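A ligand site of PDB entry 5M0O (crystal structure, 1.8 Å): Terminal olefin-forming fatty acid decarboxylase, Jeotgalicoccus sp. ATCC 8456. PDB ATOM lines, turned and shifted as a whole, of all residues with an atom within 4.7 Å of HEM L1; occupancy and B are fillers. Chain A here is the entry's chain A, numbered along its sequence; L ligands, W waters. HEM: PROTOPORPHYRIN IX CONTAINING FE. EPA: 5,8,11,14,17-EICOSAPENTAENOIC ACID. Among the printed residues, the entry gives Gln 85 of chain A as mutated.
A ring nitrogen (ND1) of His 363 sits at hydrogen-bond distance from an oxygen (O2D) of HEM L1, at 2.8 Å. An iron atom (FE) of HEM L1 is bound by the side-chain sulfur (SG) of Cys 365 (2.4 Å). An oxygen (O1A) of HEM L1 sits at hydrogen-bond distance from the side-chain hydroxyl of Tyr 59. NZ of Lys 96 is in salt-bridge range of O1D of HEM L1, 2.8 Å away. The guanidinium group (NH2) of Arg 66 lies within salt-bridge range of an oxygen (O2A) of HEM L1, at 2.7 Å. NE2 of His 92 lies within hydrogen-bond range of O1D of HEM L1 (2.7 Å).
NE2 of His 92 sits at hydrogen-bond distance from ND1 of His 363, at 3.5 Å. O of Gly 367 sits at hydrogen-bond distance from OG1 of Thr 371 (2.9 Å). ND2 of Asn 242 is in hydrogen-bond range of OE1 of Gln 85 (3.2 Å). NZ of Lys 96 sits at hydrogen-bond distance from O of Asn 362, 2.9 Å away. O of Gln 354 sits close to N of Cys 365, 3.0 Å away. The side-chain amino group (NZ) of Lys 96 lies within hydrogen-bond range of the backbone carbonyl oxygen (O) of Arg 364 (2.7 Å). OG1 of Thr 371 lies within hydrogen-bond range of OE1 of Gln 354 (3.2 Å). The backbone carbonyl oxygen (O) of Tyr 59 is in hydrogen-bond range of the side-chain amide nitrogen (ND2) of Asn 362.
The side-chain amide oxygen (OE1) of Gln 354 lies close to a nitrogen (NB) of HEM L1 (3.2 Å). CG1 of Ile 84 touches O2D of HEM L1, 3.7 Å away. NE2 of Gln 85 touches CAD of HEM L1, 3.7 Å away. Phe 99 touches HEM L1 (CD2 to CMD, 3.3 Å). Asn 242 touches HEM L1 (O to CHD, 3.5 Å). Thr 243 touches HEM L1 (O to CBC, 3.1 Å). Pro 246 touches HEM L1 (CB to C1C, 3.3 Å). Leu 247 touches HEM L1 (CA to CMC, 3.4 Å). Ala 249 touches HEM L1 (C to CBB, 3.7 Å). N of Ile 250 touches CBB of HEM L1, 3.5 Å away. Phe 253 touches HEM L1 (CE2 to CAB, 3.6 Å). CD2 of Phe 291 touches CMB of HEM L1 (3.8 Å). CG2 of Val 292 touches CMA of HEM L1 (3.7 Å). CD1 of Leu 295 touches CGA of HEM L1, 3.7 Å away. Asn 362 touches HEM L1. Arg 364 touches HEM L1. Ala 366 touches HEM L1. CA of Gly 367 touches C3C of HEM L1, 3.5 Å away. Ile 370 touches HEM L1. Thr 371 touches HEM L1. Hydrophobic or aromatic side chains within 4 Å of HEM L1: Tyr 59, Ile 84, His 92, Phe 99, Pro 246, Leu 247, Ala 249, Ile 250, Phe 253, Phe 291, Val 292, Leu 295, His 363 and Ile 370. 26 residues have an atom within 4 Å of HEM L1: Tyr 59, Arg 66, Ile 84, Gln 85, His 92, Lys 96, Phe 99, Asn 242, Thr 243, Pro 246, Leu 247, Ala 249, Ile 250, Phe 253, Phe 291, Val 292, Leu 295, Gln 354, Asn 362, His 363, Arg 364, Cys 365, Ala 366, Gly 367, Ile 370 and Thr 371.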
ATOM      1  N   TYR A  59      14.375  30.969   8.149  1.00  0.00           N
ATOM      2  CA  TYR A  59      14.224  32.045   7.174  1.00  0.00           C
ATOM      3  C   TYR A  59      13.302  33.173   7.631  1.00  0.00           C
ATOM      4  O   TYR A  59      12.884  34.019   6.826  1.00  0.00           O
ATOM      5  CB  TYR A  59      13.786  31.471   5.790  1.00  0.00           C
ATOM      6  CG  TYR A  59      14.937  30.727   5.082  1.00  0.00           C
ATOM      7  CD1 TYR A  59      16.028  31.395   4.643  1.00  0.00           C
ATOM      8  CD2 TYR A  59      14.927  29.325   4.955  1.00  0.00           C
ATOM      9  CE1 TYR A  59      17.107  30.731   4.042  1.00  0.00           C
ATOM     10  CE2 TYR A  59      15.998  28.659   4.366  1.00  0.00           C
ATOM     11  CZ  TYR A  59      17.076  29.354   3.905  1.00  0.00           C
ATOM     12  OH  TYR A  59      18.185  28.729   3.244  1.00  0.00           O
ATOM     13  N   ARG A  66      22.132  35.940   9.576  1.00  0.00           N
ATOM     14  CA  ARG A  66      23.086  35.112   8.795  1.00  0.00           C
ATOM     15  C   ARG A  66      24.434  35.743   8.681  1.00  0.00           C
ATOM     16  O   ARG A  66      25.475  35.078   8.549  1.00  0.00           O
ATOM     17  CB  ARG A  66      22.492  34.838   7.398  1.00  0.00           C
ATOM     18  CG  ARG A  66      21.103  34.178   7.429  1.00  0.00           C
ATOM     19  CD  ARG A  66      21.109  32.759   7.966  1.00  0.00           C
ATOM     20  NE  ARG A  66      21.976  31.957   7.157  1.00  0.00           N
ATOM     21  CZ  ARG A  66      21.638  31.510   5.949  1.00  0.00           C
ATOM     22  NH1 ARG A  66      20.415  31.704   5.433  1.00  0.00           N
ATOM     23  NH2 ARG A  66      22.537  30.850   5.282  1.00  0.00           N
ATOM     24  N   ILE A  84      27.608  38.729  -1.430  1.00  0.00           N
ATOM     25  CA  ILE A  84      26.190  38.754  -1.117  1.00  0.00           C
ATOM     26  C   ILE A  84      25.861  37.832   0.046  1.00  0.00           C
ATOM     27  O   ILE A  84      25.030  38.166   0.854  1.00  0.00           O
ATOM     28  CB  ILE A  84      25.267  38.448  -2.368  1.00  0.00           C
ATOM     29  CG1 ILE A  84      23.775  38.507  -2.074  1.00  0.00           C
ATOM     30  CG2 ILE A  84      25.505  37.059  -2.900  1.00  0.00           C
ATOM     31  CD1 ILE A  84      22.995  39.551  -2.777  1.00  0.00           C
ATOM     32  N   GLN A  85      26.461  36.627   0.142  1.00  0.00           N
ATOM     33  CA  GLN A  85      26.182  35.731   1.249  1.00  0.00           C
ATOM     34  C   GLN A  85      26.577  36.303   2.620  1.00  0.00           C
ATOM     35  O   GLN A  85      26.082  35.800   3.644  1.00  0.00           O
ATOM     36  CB  GLN A  85      26.948  34.409   1.073  1.00  0.00           C
ATOM     37  CG  GLN A  85      26.535  33.629  -0.176  1.00  0.00           C
ATOM     38  CD  GLN A  85      27.227  34.032  -1.474  1.00  0.00           C
ATOM     39  OE1 GLN A  85      28.004  34.989  -1.538  1.00  0.00           O
ATOM     40  NE2 GLN A  85      26.978  33.223  -2.533  1.00  0.00           N
ATOM     41  N   HIS A  92      21.365  43.772   1.569  1.00  0.00           N
ATOM     42  CA  HIS A  92      21.219  42.436   1.004  1.00  0.00           C
ATOM     43  C   HIS A  92      20.057  42.370   0.027  1.00  0.00           C
ATOM     44  O   HIS A  92      20.212  41.960  -1.108  1.00  0.00           O
ATOM     45  CB  HIS A  92      21.004  41.396   2.074  1.00  0.00           C
ATOM     46  CG  HIS A  92      20.589  40.075   1.496  1.00  0.00           C
ATOM     47  ND1 HIS A  92      19.276  39.656   1.463  1.00  0.00           N
ATOM     48  CD2 HIS A  92      21.297  39.147   0.795  1.00  0.00           C
ATOM     49  CE1 HIS A  92      19.205  38.484   0.858  1.00  0.00           C
ATOM     50  NE2 HIS A  92      20.413  38.155   0.444  1.00  0.00           N
ATOM     51  N   LYS A  96      20.420  41.587  -3.785  1.00  0.00           N
ATOM     52  CA  LYS A  96      19.790  40.319  -4.244  1.00  0.00           C
ATOM     53  C   LYS A  96      18.908  40.597  -5.503  1.00  0.00           C
ATOM     54  O   LYS A  96      18.794  39.771  -6.459  1.00  0.00           O
ATOM     55  CB  LYS A  96      19.040  39.662  -3.119  1.00  0.00           C
ATOM     56  CG  LYS A  96      18.327  38.374  -3.481  1.00  0.00           C
ATOM     57  CD  LYS A  96      19.345  37.341  -3.956  1.00  0.00           C
ATOM     58  CE  LYS A  96      18.739  35.940  -3.989  1.00  0.00           C
ATOM     59  NZ  LYS A  96      18.490  35.391  -2.640  1.00  0.00           N
ATOM     60  N   PHE A  99      20.842  40.267  -8.658  1.00  0.00           N
ATOM     61  CA  PHE A  99      21.045  38.868  -9.069  1.00  0.00           C
ATOM     62  C   PHE A  99      19.758  38.337  -9.721  1.00  0.00           C
ATOM     63  O   PHE A  99      19.807  37.722 -10.797  1.00  0.00           O
ATOM     64  CB  PHE A  99      21.467  37.979  -7.867  1.00  0.00           C
ATOM     65  CG  PHE A  99      22.946  38.049  -7.489  1.00  0.00           C
ATOM     66  CD1 PHE A  99      23.415  38.988  -6.592  1.00  0.00           C
ATOM     67  CD2 PHE A  99      23.856  37.092  -7.966  1.00  0.00           C
ATOM     68  CE1 PHE A  99      24.758  39.044  -6.262  1.00  0.00           C
ATOM     69  CE2 PHE A  99      25.214  37.129  -7.655  1.00  0.00           C
ATOM     70  CZ  PHE A  99      25.644  38.126  -6.767  1.00  0.00           C
ATOM     71  N   MET A 103      17.487  36.789 -14.240  1.00  0.00           N
ATOM     72  CA  MET A 103      16.776  35.534 -14.469  1.00  0.00           C
ATOM     73  C   MET A 103      15.481  35.799 -15.279  1.00  0.00           C
ATOM     74  O   MET A 103      14.352  35.386 -14.908  1.00  0.00           O
ATOM     75  CB  MET A 103      16.455  34.894 -13.136  1.00  0.00           C
ATOM     76  CG  MET A 103      17.694  34.665 -12.265  1.00  0.00           C
ATOM     77  SD  MET A 103      19.074  33.865 -13.034  1.00  0.00           S
ATOM     78  CE  MET A 103      20.407  34.062 -11.800  1.00  0.00           C
ATOM     79  N   TRP A 149      27.458  32.871 -20.575  1.00  0.00           N
ATOM     80  CA  TRP A 149      26.185  33.348 -20.093  1.00  0.00           C
ATOM     81  C   TRP A 149      26.399  34.649 -19.257  1.00  0.00           C
ATOM     82  O   TRP A 149      25.600  35.561 -19.316  1.00  0.00           O
ATOM     83  CB  TRP A 149      25.498  32.264 -19.228  1.00  0.00           C
ATOM     84  CG  TRP A 149      24.192  32.679 -18.732  1.00  0.00           C
ATOM     85  CD1 TRP A 149      23.053  32.735 -19.466  1.00  0.00           C
ATOM     86  CD2 TRP A 149      23.883  33.279 -17.479  1.00  0.00           C
ATOM     87  NE1 TRP A 149      22.040  33.245 -18.705  1.00  0.00           N
ATOM     88  CE2 TRP A 149      22.525  33.581 -17.491  1.00  0.00           C
ATOM     89  CE3 TRP A 149      24.607  33.469 -16.297  1.00  0.00           C
ATOM     90  CZ2 TRP A 149      21.858  34.145 -16.402  1.00  0.00           C
ATOM     91  CZ3 TRP A 149      23.962  33.973 -15.226  1.00  0.00           C
ATOM     92  CH2 TRP A 149      22.602  34.332 -15.267  1.00  0.00           C
ATOM     93  N   ASN A 242      29.836  35.022  -8.297  1.00  0.00           N
ATOM     94  CA  ASN A 242      28.717  34.313  -7.694  1.00  0.00           C
ATOM     95  C   ASN A 242      27.545  34.070  -8.658  1.00  0.00           C
ATOM     96  O   ASN A 242      26.572  33.423  -8.292  1.00  0.00           O
ATOM     97  CB  ASN A 242      28.188  35.046  -6.458  1.00  0.00           C
ATOM     98  CG  ASN A 242      29.038  34.785  -5.209  1.00  0.00           C
ATOM     99  OD1 ASN A 242      29.590  33.674  -5.039  1.00  0.00           O
ATOM    100  ND2 ASN A 242      29.240  35.812  -4.382  1.00  0.00           N
ATOM    101  N   THR A 243      27.642  34.618  -9.861  1.00  0.00           N
ATOM    102  CA  THR A 243      26.668  34.377 -10.950  1.00  0.00           C
ATOM    103  C   THR A 243      27.043  33.194 -11.808  1.00  0.00           C
ATOM    104  O   THR A 243      26.214  32.760 -12.648  1.00  0.00           O
ATOM    105  CB  THR A 243      26.488  35.610 -11.924  1.00  0.00           C
ATOM    106  OG1 THR A 243      27.654  35.801 -12.783  1.00  0.00           O
ATOM    107  CG2 THR A 243      26.044  36.807 -11.236  1.00  0.00           C
ATOM    108  N   PRO A 246      28.898  29.005  -9.183  1.00  0.00           N
ATOM    109  CA  PRO A 246      27.933  27.950  -8.787  1.00  0.00           C
ATOM    110  C   PRO A 246      27.229  27.257  -9.987  1.00  0.00           C
ATOM    111  O   PRO A 246      26.782  26.110  -9.900  1.00  0.00           O
ATOM    112  CB  PRO A 246      26.883  28.684  -7.945  1.00  0.00           C
ATOM    113  CG  PRO A 246      27.340  30.099  -7.846  1.00  0.00           C
ATOM    114  CD  PRO A 246      28.464  30.352  -8.777  1.00  0.00           C
ATOM    115  N   LEU A 247      27.188  27.940 -11.118  1.00  0.00           N
ATOM    116  CA  LEU A 247      26.793  27.304 -12.379  1.00  0.00           C
ATOM    117  C   LEU A 247      27.738  26.195 -12.742  1.00  0.00           C
ATOM    118  O   LEU A 247      27.310  25.084 -13.132  1.00  0.00           O
ATOM    119  CB  LEU A 247      26.658  28.413 -13.475  1.00  0.00           C
ATOM    120  CG  LEU A 247      25.973  28.050 -14.789  1.00  0.00           C
ATOM    121  CD1 LEU A 247      25.463  29.300 -15.501  1.00  0.00           C
ATOM    122  CD2 LEU A 247      26.834  27.200 -15.703  1.00  0.00           C
ATOM    123  N   ALA A 249      29.577  24.572 -10.718  1.00  0.00           N
ATOM    124  CA  ALA A 249      29.333  23.520  -9.676  1.00  0.00           C
ATOM    125  C   ALA A 249      28.256  22.531  -9.976  1.00  0.00           C
ATOM    126  O   ALA A 249      28.115  21.503  -9.306  1.00  0.00           O
ATOM    127  CB  ALA A 249      29.021  24.182  -8.324  1.00  0.00           C
ATOM    128  N   ILE A 250      27.379  22.885 -10.967  1.00  0.00           N
ATOM    129  CA  ILE A 250      26.434  21.910 -11.459  1.00  0.00           C
ATOM    130  C   ILE A 250      27.090  20.639 -11.914  1.00  0.00           C
ATOM    131  O   ILE A 250      26.405  19.621 -12.061  1.00  0.00           O
ATOM    132  CB  ILE A 250      25.479  22.559 -12.533  1.00  0.00           C
ATOM    133  CG1 ILE A 250      24.662  23.661 -11.915  1.00  0.00           C
ATOM    134  CG2 ILE A 250      24.490  21.556 -13.116  1.00  0.00           C
ATOM    135  CD1 ILE A 250      24.022  24.652 -12.891  1.00  0.00           C
ATOM    136  N   PHE A 253      26.209  17.723  -9.896  1.00  0.00           N
ATOM    137  CA  PHE A 253      24.859  17.176 -10.182  1.00  0.00           C
ATOM    138  C   PHE A 253      24.855  16.453 -11.503  1.00  0.00           C
ATOM    139  O   PHE A 253      24.127  15.500 -11.637  1.00  0.00           O
ATOM    140  CB  PHE A 253      23.778  18.264 -10.184  1.00  0.00           C
ATOM    141  CG  PHE A 253      23.316  18.729  -8.836  1.00  0.00           C
ATOM    142  CD1 PHE A 253      23.219  17.856  -7.752  1.00  0.00           C
ATOM    143  CD2 PHE A 253      23.021  20.048  -8.623  1.00  0.00           C
ATOM    144  CE1 PHE A 253      22.821  18.298  -6.527  1.00  0.00           C
ATOM    145  CE2 PHE A 253      22.554  20.516  -7.389  1.00  0.00           C
ATOM    146  CZ  PHE A 253      22.432  19.630  -6.323  1.00  0.00           C
ATOM    147  N   PHE A 291      24.835  17.435  -1.344  1.00  0.00           N
ATOM    148  CA  PHE A 291      25.729  18.523  -1.707  1.00  0.00           C
ATOM    149  C   PHE A 291      25.903  19.436  -0.513  1.00  0.00           C
ATOM    150  O   PHE A 291      26.986  19.370   0.157  1.00  0.00           O
ATOM    151  CB  PHE A 291      25.224  19.244  -2.994  1.00  0.00           C
ATOM    152  CG  PHE A 291      26.281  20.105  -3.695  1.00  0.00           C
ATOM    153  CD1 PHE A 291      27.170  20.874  -3.020  1.00  0.00           C
ATOM    154  CD2 PHE A 291      26.269  20.214  -5.050  1.00  0.00           C
ATOM    155  CE1 PHE A 291      28.115  21.692  -3.697  1.00  0.00           C
ATOM    156  CE2 PHE A 291      27.169  21.010  -5.744  1.00  0.00           C
ATOM    157  CZ  PHE A 291      28.073  21.761  -5.087  1.00  0.00           C
ATOM    158  N   VAL A 292      24.880  20.249  -0.213  1.00  0.00           N
ATOM    159  CA  VAL A 292      24.941  21.166   0.932  1.00  0.00           C
ATOM    160  C   VAL A 292      24.497  20.440   2.207  1.00  0.00           C
ATOM    161  O   VAL A 292      23.423  19.909   2.223  1.00  0.00           O
ATOM    162  CB  VAL A 292      24.001  22.335   0.710  1.00  0.00           C
ATOM    163  CG1 VAL A 292      24.059  23.278   1.924  1.00  0.00           C
ATOM    164  CG2 VAL A 292      24.436  23.071  -0.561  1.00  0.00           C
ATOM    165  N   LEU A 295      23.286  24.825   6.850  1.00  0.00           N
ATOM    166  CA  LEU A 295      23.563  26.255   6.739  1.00  0.00           C
ATOM    167  C   LEU A 295      23.570  26.919   8.140  1.00  0.00           C
ATOM    168  O   LEU A 295      22.739  26.586   8.938  1.00  0.00           O
ATOM    169  CB  LEU A 295      22.499  26.906   5.866  1.00  0.00           C
ATOM    170  CG  LEU A 295      22.533  26.412   4.413  1.00  0.00           C
ATOM    171  CD1 LEU A 295      21.283  26.903   3.678  1.00  0.00           C
ATOM    172  CD2 LEU A 295      23.788  26.855   3.677  1.00  0.00           C
ATOM    173  N   PRO A 353      17.508  21.946  -1.230  1.00  0.00           N
ATOM    174  CA  PRO A 353      18.955  21.644  -1.415  1.00  0.00           C
ATOM    175  C   PRO A 353      19.825  22.861  -1.742  1.00  0.00           C
ATOM    176  O   PRO A 353      21.073  22.783  -1.654  1.00  0.00           O
ATOM    177  CB  PRO A 353      18.946  20.740  -2.651  1.00  0.00           C
ATOM    178  CG  PRO A 353      17.697  21.174  -3.410  1.00  0.00           C
ATOM    179  CD  PRO A 353      16.691  21.448  -2.360  1.00  0.00           C
ATOM    180  N   GLN A 354      19.179  23.947  -2.181  1.00  0.00           N
ATOM    181  CA  GLN A 354      19.902  25.199  -2.490  1.00  0.00           C
ATOM    182  C   GLN A 354      19.324  26.327  -1.644  1.00  0.00           C
ATOM    183  O   GLN A 354      19.180  27.494  -2.074  1.00  0.00           O
ATOM    184  CB  GLN A 354      19.866  25.512  -4.023  1.00  0.00           C
ATOM    185  CG  GLN A 354      20.419  24.357  -4.828  1.00  0.00           C
ATOM    186  CD  GLN A 354      20.439  24.515  -6.336  1.00  0.00           C
ATOM    187  OE1 GLN A 354      20.801  25.564  -6.942  1.00  0.00           O
ATOM    188  NE2 GLN A 354      20.134  23.460  -6.970  1.00  0.00           N
ATOM    189  N   GLY A 355      18.894  25.951  -0.426  1.00  0.00           N
ATOM    190  CA  GLY A 355      18.148  26.850   0.433  1.00  0.00           C
ATOM    191  C   GLY A 355      16.661  26.874   0.351  1.00  0.00           C
ATOM    192  O   GLY A 355      16.035  26.336  -0.555  1.00  0.00           O
ATOM    193  N   ASN A 362      15.293  36.526   1.386  1.00  0.00           N
ATOM    194  CA  ASN A 362      16.155  35.582   2.054  1.00  0.00           C
ATOM    195  C   ASN A 362      17.417  35.258   1.242  1.00  0.00           C
ATOM    196  O   ASN A 362      17.512  35.641   0.086  1.00  0.00           O
ATOM    197  CB  ASN A 362      15.381  34.248   2.344  1.00  0.00           C
ATOM    198  CG  ASN A 362      14.288  34.393   3.371  1.00  0.00           C
ATOM    199  OD1 ASN A 362      13.137  34.050   3.123  1.00  0.00           O
ATOM    200  ND2 ASN A 362      14.660  34.877   4.581  1.00  0.00           N
ATOM    201  N   HIS A 363      18.376  34.551   1.851  1.00  0.00           N
ATOM    202  CA  HIS A 363      19.604  34.149   1.186  1.00  0.00           C
ATOM    203  C   HIS A 363      19.449  32.939   0.222  1.00  0.00           C
ATOM    204  O   HIS A 363      20.446  32.399  -0.238  1.00  0.00           O
ATOM    205  CB  HIS A 363      20.746  33.851   2.197  1.00  0.00           C
ATOM    206  CG  HIS A 363      21.355  35.081   2.798  1.00  0.00           C
ATOM    207  ND1 HIS A 363      22.317  35.801   2.136  1.00  0.00           N
ATOM    208  CD2 HIS A 363      21.066  35.765   3.930  1.00  0.00           C
ATOM    209  CE1 HIS A 363      22.653  36.843   2.865  1.00  0.00           C
ATOM    210  NE2 HIS A 363      21.902  36.853   3.947  1.00  0.00           N
ATOM    211  N   ARG A 364      18.209  32.558  -0.089  1.00  0.00           N
ATOM    212  CA  ARG A 364      17.912  31.411  -0.977  1.00  0.00           C
ATOM    213  C   ARG A 364      18.644  31.563  -2.331  1.00  0.00           C
ATOM    214  O   ARG A 364      18.766  32.673  -2.841  1.00  0.00           O
ATOM    215  CB  ARG A 364      16.398  31.364  -1.247  1.00  0.00           C
ATOM    216  CG  ARG A 364      15.946  30.161  -2.074  1.00  0.00           C
ATOM    217  CD  ARG A 364      14.452  30.101  -2.341  1.00  0.00           C
ATOM    218  NE  ARG A 364      14.081  28.848  -2.976  1.00  0.00           N
ATOM    219  CZ  ARG A 364      13.275  27.913  -2.460  1.00  0.00           C
ATOM    220  NH1 ARG A 364      12.606  28.103  -1.301  1.00  0.00           N
ATOM    221  NH2 ARG A 364      13.146  26.756  -3.102  1.00  0.00           N
ATOM    222  N   CYS A 365      19.128  30.432  -2.865  1.00  0.00           N
ATOM    223  CA  CYS A 365      19.835  30.416  -4.138  1.00  0.00           C
ATOM    224  C   CYS A 365      19.097  31.178  -5.241  1.00  0.00           C
ATOM    225  O   CYS A 365      17.910  30.958  -5.463  1.00  0.00           O
ATOM    226  CB  CYS A 365      19.983  28.961  -4.551  1.00  0.00           C
ATOM    227  SG  CYS A 365      20.964  28.754  -6.052  1.00  0.00           S
ATOM    228  N   ALA A 366      19.820  32.067  -5.929  1.00  0.00           N
ATOM    229  CA  ALA A 366      19.243  32.754  -7.114  1.00  0.00           C
ATOM    230  C   ALA A 366      19.254  31.904  -8.374  1.00  0.00           C
ATOM    231  O   ALA A 366      18.682  32.311  -9.396  1.00  0.00           O
ATOM    232  CB  ALA A 366      20.013  34.038  -7.405  1.00  0.00           C
ATOM    233  N   GLY A 367      19.936  30.767  -8.300  1.00  0.00           N
ATOM    234  CA  GLY A 367      20.264  29.979  -9.497  1.00  0.00           C
ATOM    235  C   GLY A 367      19.478  28.717  -9.648  1.00  0.00           C
ATOM    236  O   GLY A 367      19.854  27.867 -10.429  1.00  0.00           O
ATOM    237  N   ILE A 370      18.245  28.105 -13.296  1.00  0.00           N
ATOM    238  CA  ILE A 370      19.348  27.752 -14.123  1.00  0.00           C
ATOM    239  C   ILE A 370      19.821  26.304 -13.869  1.00  0.00           C
ATOM    240  O   ILE A 370      20.122  25.564 -14.839  1.00  0.00           O
ATOM    241  CB  ILE A 370      20.506  28.729 -13.959  1.00  0.00           C
ATOM    242  CG1 ILE A 370      20.165  30.042 -14.628  1.00  0.00           C
ATOM    243  CG2 ILE A 370      21.825  28.196 -14.495  1.00  0.00           C
ATOM    244  CD1 ILE A 370      21.174  31.091 -14.332  1.00  0.00           C
ATOM    245  N   THR A 371      19.906  25.915 -12.594  1.00  0.00           N
ATOM    246  CA  THR A 371      20.366  24.563 -12.252  1.00  0.00           C
ATOM    247  C   THR A 371      19.445  23.533 -12.940  1.00  0.00           C
ATOM    248  O   THR A 371      19.933  22.530 -13.496  1.00  0.00           O
ATOM    249  CB  THR A 371      20.371  24.366 -10.716  1.00  0.00           C
ATOM    250  OG1 THR A 371      21.281  25.330 -10.147  1.00  0.00           O
ATOM    251  CG2 THR A 371      20.930  23.018 -10.300  1.00  0.00           C
HETATM  252  CHA HEM L   1      22.950  30.860  -2.610  1.00  0.00           C
HETATM  253  CHB HEM L   1      23.412  26.059  -3.390  1.00  0.00           C
HETATM  254  CHC HEM L   1      23.738  26.937  -8.137  1.00  0.00           C
HETATM  255  CHD HEM L   1      23.672  31.669  -7.309  1.00  0.00           C
HETATM  256  C1A HEM L   1      22.942  29.494  -2.467  1.00  0.00           C
HETATM  257  C2A HEM L   1      22.857  28.844  -1.176  1.00  0.00           C
HETATM  258  C3A HEM L   1      23.007  27.513  -1.393  1.00  0.00           C
HETATM  259  C4A HEM L   1      23.144  27.297  -2.803  1.00  0.00           C
HETATM  260  CMA HEM L   1      22.978  26.446  -0.305  1.00  0.00           C
HETATM  261  CAA HEM L   1      22.686  29.601   0.179  1.00  0.00           C
HETATM  262  CBA HEM L   1      21.242  29.551   0.721  1.00  0.00           C
HETATM  263  CGA HEM L   1      21.191  30.285   2.067  1.00  0.00           C
HETATM  264  O1A HEM L   1      20.116  30.390   2.735  1.00  0.00           O
HETATM  265  O2A HEM L   1      22.253  30.773   2.556  1.00  0.00           O
HETATM  266  C1B HEM L   1      23.666  25.923  -4.764  1.00  0.00           C
HETATM  267  C2B HEM L   1      23.905  24.666  -5.338  1.00  0.00           C
HETATM  268  C3B HEM L   1      24.023  24.875  -6.655  1.00  0.00           C
HETATM  269  C4B HEM L   1      23.798  26.322  -6.899  1.00  0.00           C
HETATM  270  CMB HEM L   1      24.119  23.343  -4.592  1.00  0.00           C
HETATM  271  CAB HEM L   1      24.385  23.665  -7.381  1.00  0.00           C
HETATM  272  CBB HEM L   1      25.140  23.664  -8.357  1.00  0.00           C
HETATM  273  C1C HEM L   1      23.652  28.248  -8.357  1.00  0.00           C
HETATM  274  C2C HEM L   1      23.733  28.825  -9.643  1.00  0.00           C
HETATM  275  C3C HEM L   1      23.733  30.209  -9.372  1.00  0.00           C
HETATM  276  C4C HEM L   1      23.667  30.428  -7.965  1.00  0.00           C
HETATM  277  CMC HEM L   1      23.772  28.106 -11.004  1.00  0.00           C
HETATM  278  CAC HEM L   1      23.827  31.288 -10.313  1.00  0.00           C
HETATM  279  CBC HEM L   1      23.828  31.095 -11.606  1.00  0.00           C
HETATM  280  C1D HEM L   1      23.562  31.785  -5.928  1.00  0.00           C
HETATM  281  C2D HEM L   1      23.547  33.117  -5.299  1.00  0.00           C
HETATM  282  C3D HEM L   1      23.344  32.889  -3.989  1.00  0.00           C
HETATM  283  C4D HEM L   1      23.204  31.427  -3.851  1.00  0.00           C
HETATM  284  CMD HEM L   1      23.774  34.429  -5.952  1.00  0.00           C
HETATM  285  CAD HEM L   1      23.315  33.913  -2.863  1.00  0.00           C
HETATM  286  CBD HEM L   1      21.949  34.496  -2.641  1.00  0.00           C
HETATM  287  CGD HEM L   1      21.894  35.290  -1.332  1.00  0.00           C
HETATM  288  O1D HEM L   1      20.813  35.961  -1.106  1.00  0.00           O
HETATM  289  O2D HEM L   1      22.909  35.287  -0.529  1.00  0.00           O
HETATM  290  NA  HEM L   1      23.118  28.561  -3.424  1.00  0.00           N
HETATM  291  NB  HEM L   1      23.473  26.839  -5.735  1.00  0.00           N
HETATM  292  NC  HEM L   1      23.568  29.213  -7.411  1.00  0.00           N
HETATM  293  ND  HEM L   1      23.222  30.814  -5.067  1.00  0.00           N
HETATM  294 FE   HEM L   1      23.292  28.889  -5.396  1.00  0.00          FE
HETATM  295  C1  EPA L   2      28.985  27.734  -5.159  1.00  0.00           C
HETATM  296  OA  EPA L   2      28.630  28.723  -4.466  1.00  0.00           O
HETATM  297  OB  EPA L   2      30.104  27.567  -5.705  1.00  0.00           O
HETATM  298  C2  EPA L   2      28.000  26.602  -5.323  1.00  0.00           C
HETATM  299  C3  EPA L   2      28.298  25.562  -4.256  1.00  0.00           C
HETATM  300  C4  EPA L   2      27.016  25.310  -3.480  1.00  0.00           C
HETATM  301  C5  EPA L   2      27.051  26.049  -2.162  1.00  0.00           C
HETATM  302  C6  EPA L   2      27.841  25.221  -1.169  1.00  0.00           C
HETATM  303  C7  EPA L   2      27.340  25.667   0.193  1.00  0.00           C
HETATM  304  C8  EPA L   2      28.103  24.987   1.332  1.00  0.00           C
HETATM  305  C9  EPA L   2      27.875  25.789   2.604  1.00  0.00           C
HETATM  306  C10 EPA L   2      28.361  24.978   3.791  1.00  0.00           C
HETATM  307  C11 EPA L   2      28.498  25.848   5.014  1.00  0.00           C
HETATM  308  C12 EPA L   2      28.590  25.006   6.286  1.00  0.00           C
HETATM  309  C13 EPA L   2      28.900  25.822   7.523  1.00  0.00           C
HETATM  310  C14 EPA L   2      29.054  24.948   8.764  1.00  0.00           C
HETATM  311  C15 EPA L   2      28.252  25.423   9.965  1.00  0.00           C
HETATM  312  C16 EPA L   2      28.343  24.423  11.106  1.00  0.00           C
HETATM  313  C17 EPA L   2      27.336  23.594  11.427  1.00  0.00           C
HETATM  314  C18 EPA L   2      27.531  22.659  12.593  1.00  0.00           C
HETATM  315  C19 EPA L   2      26.733  21.424  12.565  1.00  0.00           C
HETATM  316  C20 EPA L   2      26.087  20.297  12.625  1.00  0.00           C
HETATM  317  O   HOH W   1      25.657  29.147  -4.615  1.00  0.00           O
HETATM  318  O   HOH W   2      23.846  32.741   1.363  1.00  0.00           O
